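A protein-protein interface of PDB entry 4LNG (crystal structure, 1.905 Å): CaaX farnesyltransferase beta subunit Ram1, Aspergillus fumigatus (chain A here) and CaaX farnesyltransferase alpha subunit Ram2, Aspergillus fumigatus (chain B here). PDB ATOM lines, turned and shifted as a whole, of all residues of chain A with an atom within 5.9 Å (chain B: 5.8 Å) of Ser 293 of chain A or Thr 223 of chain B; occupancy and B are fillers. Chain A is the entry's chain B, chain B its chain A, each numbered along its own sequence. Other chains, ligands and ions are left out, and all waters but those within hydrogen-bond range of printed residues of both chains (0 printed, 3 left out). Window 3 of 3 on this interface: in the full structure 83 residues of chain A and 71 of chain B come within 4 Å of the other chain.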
ATOM      1  N   LEU A 288      17.332 -11.299  27.926  1.00  0.00           N
ATOM      2  CA  LEU A 288      16.322 -11.400  26.872  1.00  0.00           C
ATOM      3  C   LEU A 288      16.823 -11.104  25.447  1.00  0.00           C
ATOM      4  O   LEU A 288      16.586 -11.902  24.542  1.00  0.00           O
ATOM      5  CB  LEU A 288      15.098 -10.538  27.208  1.00  0.00           C
ATOM      6  CG  LEU A 288      13.995 -10.506  26.154  1.00  0.00           C
ATOM      7  CD1 LEU A 288      13.430 -11.907  25.933  1.00  0.00           C
ATOM      8  CD2 LEU A 288      12.901  -9.532  26.570  1.00  0.00           C
ATOM      9  N   PRO A 289      17.509  -9.963  25.234  1.00  0.00           N
ATOM     10  CA  PRO A 289      17.964  -9.738  23.856  1.00  0.00           C
ATOM     11  C   PRO A 289      19.027 -10.750  23.427  1.00  0.00           C
ATOM     12  O   PRO A 289      19.123 -11.058  22.239  1.00  0.00           O
ATOM     13  CB  PRO A 289      18.542  -8.319  23.900  1.00  0.00           C
ATOM     14  CG  PRO A 289      18.928  -8.113  25.325  1.00  0.00           C
ATOM     15  CD  PRO A 289      17.900  -8.857  26.129  1.00  0.00           C
ATOM     16  N   GLU A 290      19.803 -11.260  24.382  1.00  0.00           N
ATOM     17  CA  GLU A 290      20.769 -12.321  24.103  1.00  0.00           C
ATOM     18  C   GLU A 290      20.058 -13.601  23.666  1.00  0.00           C
ATOM     19  O   GLU A 290      20.474 -14.256  22.711  1.00  0.00           O
ATOM     20  CB  GLU A 290      21.653 -12.597  25.325  1.00  0.00           C
ATOM     21  CG  GLU A 290      22.582 -11.446  25.706  1.00  0.00           C
ATOM     22  CD  GLU A 290      21.904 -10.399  26.577  1.00  0.00           C
ATOM     23  OE1 GLU A 290      20.691 -10.532  26.845  1.00  0.00           O
ATOM     24  OE2 GLU A 290      22.589  -9.444  27.001  1.00  0.00           O
ATOM     25  N   TYR A 291      18.985 -13.948  24.372  1.00  0.00           N
ATOM     26  CA  TYR A 291      18.131 -15.065  23.981  1.00  0.00           C
ATOM     27  C   TYR A 291      17.602 -14.895  22.558  1.00  0.00           C
ATOM     28  O   TYR A 291      17.652 -15.825  21.753  1.00  0.00           O
ATOM     29  CB  TYR A 291      16.965 -15.208  24.965  1.00  0.00           C
ATOM     30  CG  TYR A 291      15.832 -16.089  24.479  1.00  0.00           C
ATOM     31  CD1 TYR A 291      15.929 -17.477  24.533  1.00  0.00           C
ATOM     32  CD2 TYR A 291      14.658 -15.532  23.986  1.00  0.00           C
ATOM     33  CE1 TYR A 291      14.886 -18.285  24.098  1.00  0.00           C
ATOM     34  CE2 TYR A 291      13.616 -16.328  23.549  1.00  0.00           C
ATOM     35  CZ  TYR A 291      13.731 -17.700  23.610  1.00  0.00           C
ATOM     36  OH  TYR A 291      12.690 -18.489  23.172  1.00  0.00           O
ATOM     37  N   LEU A 292      17.093 -13.707  22.246  1.00  0.00           N
ATOM     38  CA  LEU A 292      16.576 -13.442  20.903  1.00  0.00           C
ATOM     39  C   LEU A 292      17.671 -13.547  19.837  1.00  0.00           C
ATOM     40  O   LEU A 292      17.431 -14.049  18.740  1.00  0.00           O
ATOM     41  CB  LEU A 292      15.883 -12.074  20.852  1.00  0.00           C
ATOM     42  CG  LEU A 292      14.676 -11.963  21.786  1.00  0.00           C
ATOM     43  CD1 LEU A 292      14.115 -10.547  21.799  1.00  0.00           C
ATOM     44  CD2 LEU A 292      13.596 -12.965  21.389  1.00  0.00           C
ATOM     45  N   SER A 293      18.873 -13.080  20.165  1.00  0.00           N
ATOM     46  CA  SER A 293      20.013 -13.200  19.260  1.00  0.00           C
ATOM     47  C   SER A 293      20.319 -14.662  18.937  1.00  0.00           C
ATOM     48  O   SER A 293      20.692 -14.997  17.806  1.00  0.00           O
ATOM     49  CB  SER A 293      21.254 -12.534  19.860  1.00  0.00           C
ATOM     50  OG  SER A 293      22.416 -12.859  19.114  1.00  0.00           O
ATOM     51  N   ARG A 294      20.151 -15.531  19.930  1.00  0.00           N
ATOM     52  CA  ARG A 294      20.415 -16.960  19.747  1.00  0.00           C
ATOM     53  C   ARG A 294      19.311 -17.658  18.953  1.00  0.00           C
ATOM     54  O   ARG A 294      19.398 -18.857  18.674  1.00  0.00           O
ATOM     55  CB  ARG A 294      20.632 -17.656  21.092  1.00  0.00           C
ATOM     56  CG  ARG A 294      21.833 -17.138  21.872  1.00  0.00           C
ATOM     57  CD  ARG A 294      22.175 -18.060  23.038  1.00  0.00           C
ATOM     58  NE  ARG A 294      21.026 -18.291  23.909  1.00  0.00           N
ATOM     59  CZ  ARG A 294      20.702 -17.526  24.949  1.00  0.00           C
ATOM     60  NH1 ARG A 294      21.441 -16.469  25.257  1.00  0.00           N
ATOM     61  NH2 ARG A 294      19.638 -17.819  25.681  1.00  0.00           N
ATOM     62  N   CYS A 295      18.279 -16.904  18.585  1.00  0.00           N
ATOM     63  CA  CYS A 295      17.220 -17.437  17.734  1.00  0.00           C
ATOM     64  C   CYS A 295      17.389 -17.072  16.259  1.00  0.00           C
ATOM     65  O   CYS A 295      16.620 -17.529  15.417  1.00  0.00           O
ATOM     66  CB  CYS A 295      15.836 -17.011  18.236  1.00  0.00           C
ATOM     67  SG  CYS A 295      15.358 -17.785  19.806  1.00  0.00           S
ATOM     68  N   GLN A 296      18.384 -16.251  15.932  1.00  0.00           N
ATOM     69  CA  GLN A 296      18.652 -15.999  14.520  1.00  0.00           C
ATOM     70  C   GLN A 296      19.247 -17.267  13.909  1.00  0.00           C
ATOM     71  O   GLN A 296      19.933 -18.024  14.596  1.00  0.00           O
ATOM     72  CB  GLN A 296      19.577 -14.794  14.310  1.00  0.00           C
ATOM     73  CG  GLN A 296      19.664 -14.368  12.839  1.00  0.00           C
ATOM     74  CD  GLN A 296      20.326 -13.015  12.632  1.00  0.00           C
ATOM     75  OE1 GLN A 296      21.127 -12.561  13.454  1.00  0.00           O
ATOM     76  NE2 GLN A 296      19.987 -12.361  11.524  1.00  0.00           N
ATOM     77  N   ARG A 334      22.559  -4.500  17.054  1.00  0.00           N
ATOM     78  CA  ARG A 334      23.409  -5.059  18.096  1.00  0.00           C
ATOM     79  C   ARG A 334      23.186  -6.558  18.279  1.00  0.00           C
ATOM     80  O   ARG A 334      24.138  -7.319  18.468  1.00  0.00           O
ATOM     81  CB  ARG A 334      23.198  -4.335  19.431  1.00  0.00           C
ATOM     82  CG  ARG A 334      24.077  -4.891  20.544  1.00  0.00           C
ATOM     83  CD  ARG A 334      23.944  -4.111  21.840  1.00  0.00           C
ATOM     84  NE  ARG A 334      24.868  -4.613  22.855  1.00  0.00           N
ATOM     85  CZ  ARG A 334      24.947  -4.142  24.097  1.00  0.00           C
ATOM     86  NH1 ARG A 334      24.152  -3.156  24.488  1.00  0.00           N
ATOM     87  NH2 ARG A 334      25.820  -4.662  24.950  1.00  0.00           N
ATOM     88  N   TYR A 335      21.930  -6.984  18.216  1.00  0.00           N
ATOM     89  CA  TYR A 335      21.600  -8.371  18.530  1.00  0.00           C
ATOM     90  C   TYR A 335      21.281  -9.236  17.312  1.00  0.00           C
ATOM     91  O   TYR A 335      21.313 -10.464  17.397  1.00  0.00           O
ATOM     92  CB  TYR A 335      20.475  -8.431  19.571  1.00  0.00           C
ATOM     93  CG  TYR A 335      20.894  -7.818  20.886  1.00  0.00           C
ATOM     94  CD1 TYR A 335      21.737  -8.503  21.752  1.00  0.00           C
ATOM     95  CD2 TYR A 335      20.472  -6.545  21.251  1.00  0.00           C
ATOM     96  CE1 TYR A 335      22.138  -7.946  22.951  1.00  0.00           C
ATOM     97  CE2 TYR A 335      20.869  -5.978  22.451  1.00  0.00           C
ATOM     98  CZ  TYR A 335      21.702  -6.685  23.294  1.00  0.00           C
ATOM     99  OH  TYR A 335      22.104  -6.133  24.488  1.00  0.00           O
ATOM    100  N   MET A 336      20.994  -8.596  16.183  1.00  0.00           N
ATOM    101  CA  MET A 336      20.733  -9.314  14.937  1.00  0.00           C
ATOM    102  C   MET A 336      21.738  -8.937  13.852  1.00  0.00           C
ATOM    103  O   MET A 336      22.155  -7.784  13.755  1.00  0.00           O
ATOM    104  CB  MET A 336      19.320  -9.017  14.427  1.00  0.00           C
ATOM    105  CG  MET A 336      18.204  -9.516  15.327  1.00  0.00           C
ATOM    106  SD  MET A 336      18.235 -11.312  15.534  1.00  0.00           S
ATOM    107  CE  MET A 336      17.031 -11.511  16.844  1.00  0.00           C
ATOM    108  N   ALA B 218      21.811 -22.263  20.928  1.00  0.00           N
ATOM    109  CA  ALA B 218      21.808 -21.192  19.940  1.00  0.00           C
ATOM    110  C   ALA B 218      21.744 -21.790  18.543  1.00  0.00           C
ATOM    111  O   ALA B 218      22.205 -22.905  18.324  1.00  0.00           O
ATOM    112  CB  ALA B 218      23.052 -20.324  20.089  1.00  0.00           C
ATOM    113  N   LEU B 220      23.263 -20.365  16.054  1.00  0.00           N
ATOM    114  CA  LEU B 220      24.553 -20.029  15.462  1.00  0.00           C
ATOM    115  C   LEU B 220      25.634 -19.904  16.529  1.00  0.00           C
ATOM    116  O   LEU B 220      25.359 -19.505  17.664  1.00  0.00           O
ATOM    117  CB  LEU B 220      24.453 -18.708  14.687  1.00  0.00           C
ATOM    118  CG  LEU B 220      23.538 -18.672  13.459  1.00  0.00           C
ATOM    119  CD1 LEU B 220      23.308 -17.235  12.997  1.00  0.00           C
ATOM    120  CD2 LEU B 220      24.129 -19.505  12.327  1.00  0.00           C
ATOM    121  N   HIS B 221      26.861 -20.251  16.159  1.00  0.00           N
ATOM    122  CA  HIS B 221      28.024 -19.972  16.995  1.00  0.00           C
ATOM    123  C   HIS B 221      28.263 -18.471  17.106  1.00  0.00           C
ATOM    124  O   HIS B 221      27.744 -17.691  16.306  1.00  0.00           O
ATOM    125  CB  HIS B 221      29.277 -20.615  16.399  1.00  0.00           C
ATOM    126  CG  HIS B 221      29.409 -22.077  16.690  1.00  0.00           C
ATOM    127  ND1 HIS B 221      28.855 -23.050  15.887  1.00  0.00           N
ATOM    128  CD2 HIS B 221      30.035 -22.731  17.697  1.00  0.00           C
ATOM    129  CE1 HIS B 221      29.138 -24.241  16.383  1.00  0.00           C
ATOM    130  NE2 HIS B 221      29.852 -24.076  17.482  1.00  0.00           N
ATOM    131  N   ASN B 222      29.052 -18.083  18.105  1.00  0.00           N
ATOM    132  CA  ASN B 222      29.575 -16.722  18.221  1.00  0.00           C
ATOM    133  C   ASN B 222      28.523 -15.624  18.408  1.00  0.00           C
ATOM    134  O   ASN B 222      28.685 -14.516  17.901  1.00  0.00           O
ATOM    135  CB  ASN B 222      30.476 -16.395  17.021  1.00  0.00           C
ATOM    136  CG  ASN B 222      31.451 -15.268  17.310  1.00  0.00           C
ATOM    137  OD1 ASN B 222      31.864 -15.069  18.450  1.00  0.00           O
ATOM    138  ND2 ASN B 222      31.816 -14.519  16.275  1.00  0.00           N
ATOM    139  N   THR B 223      27.456 -15.921  19.145  1.00  0.00           N
ATOM    140  CA  THR B 223      26.441 -14.906  19.432  1.00  0.00           C
ATOM    141  C   THR B 223      26.918 -13.895  20.479  1.00  0.00           C
ATOM    142  O   THR B 223      26.259 -12.883  20.718  1.00  0.00           O
ATOM    143  CB  THR B 223      25.107 -15.532  19.895  1.00  0.00           C
ATOM    144  OG1 THR B 223      25.344 -16.387  21.019  1.00  0.00           O
ATOM    145  CG2 THR B 223      24.474 -16.339  18.768  1.00  0.00           C
ATOM    146  N   THR B 224      28.059 -14.172  21.101  1.00  0.00           N
ATOM    147  CA  THR B 224      28.638 -13.251  22.076  1.00  0.00           C
ATOM    148  C   THR B 224      29.495 -12.190  21.391  1.00  0.00           C
ATOM    149  O   THR B 224      29.864 -11.189  22.002  1.00  0.00           O
ATOM    150  CB  THR B 224      29.495 -13.989  23.126  1.00  0.00           C
ATOM    151  OG1 THR B 224      30.480 -14.790  22.461  1.00  0.00           O
ATOM    152  CG2 THR B 224      28.625 -14.885  23.997  1.00  0.00           C
ATOM    153  N   GLY B 225      29.809 -12.418  20.119  1.00  0.00           N
ATOM    154  CA  GLY B 225      30.623 -11.485  19.358  1.00  0.00           C
ATOM    155  C   GLY B 225      29.788 -10.475  18.596  1.00  0.00           C
ATOM    156  O   GLY B 225      28.572 -10.403  18.789  1.00  0.00           O
ATOM    157  N   LYS B 230      28.294 -13.310  13.602  1.00  0.00           N
ATOM    158  CA  LYS B 230      27.454 -14.375  14.140  1.00  0.00           C
ATOM    159  C   LYS B 230      27.511 -15.584  13.208  1.00  0.00           C
ATOM    160  O   LYS B 230      27.351 -15.445  11.995  1.00  0.00           O
ATOM    161  CB  LYS B 230      26.010 -13.903  14.329  1.00  0.00           C
ATOM    162  CG  LYS B 230      25.171 -14.856  15.169  1.00  0.00           C
ATOM    163  CD  LYS B 230      23.704 -14.446  15.230  1.00  0.00           C
ATOM    164  CE  LYS B 230      23.506 -13.124  15.957  1.00  0.00           C
ATOM    165  NZ  LYS B 230      22.053 -12.840  16.144  1.00  0.00           N
ATOM    166  N   GLY B 231      27.769 -16.759  13.774  1.00  0.00           N
ATOM    167  CA  GLY B 231      27.896 -17.973  12.983  1.00  0.00           C
ATOM    168  C   GLY B 231      29.311 -18.522  12.888  1.00  0.00           C
ATOM    169  O   GLY B 231      29.499 -19.715  12.647  1.00  0.00           O
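Ser 293 of chain A touches two residues of chain B. Printed residues of chain B within 4 Å of Arg 294 of chain A: Ala 218 (3.6 Å) and Thr 223 (3.7 Å). Arg 334 of chain A touches none of the printed residues of chain B. Printed residues of chain B within 4 Å of Met 336 of chain A: Lys 230 (3.95 Å). Of the printed residues of chain A, Thr 223 of chain B touches Ser 293 and Arg 294. Of the printed residues of chain A, Lys 230 of chain B touches Ser 293, Gln 296, Tyr 335 and Met 336. The nearest printed residue of chain B that does not touch Ser 293 of chain A is Leu 220 of chain B (5.9 Å).
Of the 9 printed residues of chain B, 4 touch a printed residue of chain A. Printed residues of chain B that touch a printed residue of chain A: Ala 218, Leu 220, Thr 223 and Lys 230. Printed residues of chain A that touch a printed residue of chain B: Ser 293, Arg 294, Gln 296, Tyr 335 and Met 336. Among the printed residues, no Asp or Glu carboxylate lies within 4 Å of a Lys or Arg side-chain nitrogen of the other chain.
The side-chain amino group (NZ) of Lys 230 of chain B sits at hydrogen-bond distance from the side-chain hydroxyl (OG) of Ser 293 of chain A. The side-chain amino group (NZ) of Lys 230 of chain B sits at hydrogen-bond distance from the side-chain amide oxygen (OE1) of Gln 296 of chain A. The side-chain amino group of Lys 230 of chain B is in hydrogen-bond range of the backbone carbonyl oxygen of Tyr 335 of chain A, at 2.8 Å.
The side-chain hydroxyl (OG) of Ser 293 of chain A lies within hydrogen-bond range of the backbone carbonyl oxygen (O) of Tyr 335 of chain A (3.1 Å). The side-chain sulfur (SD) of Met 336 of chain A sits close to the side-chain amide oxygen (OE1) of Gln 296 of chain A, at 3.8 Å.
Among the printed residues, merely in contact across the chains: Arg 294 of chain A with Ala 218 of chain B (3.6 Å), Arg 294 of chain A with Thr 223 of chain B (3.7 Å), Gln 296 of chain A with Leu 220 of chain B (3.8 Å), Ser 293 of chain A with Thr 223 of chain B (3.9 Å) and Met 336 of chain A with Lys 230 of chain B (3.95 Å).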
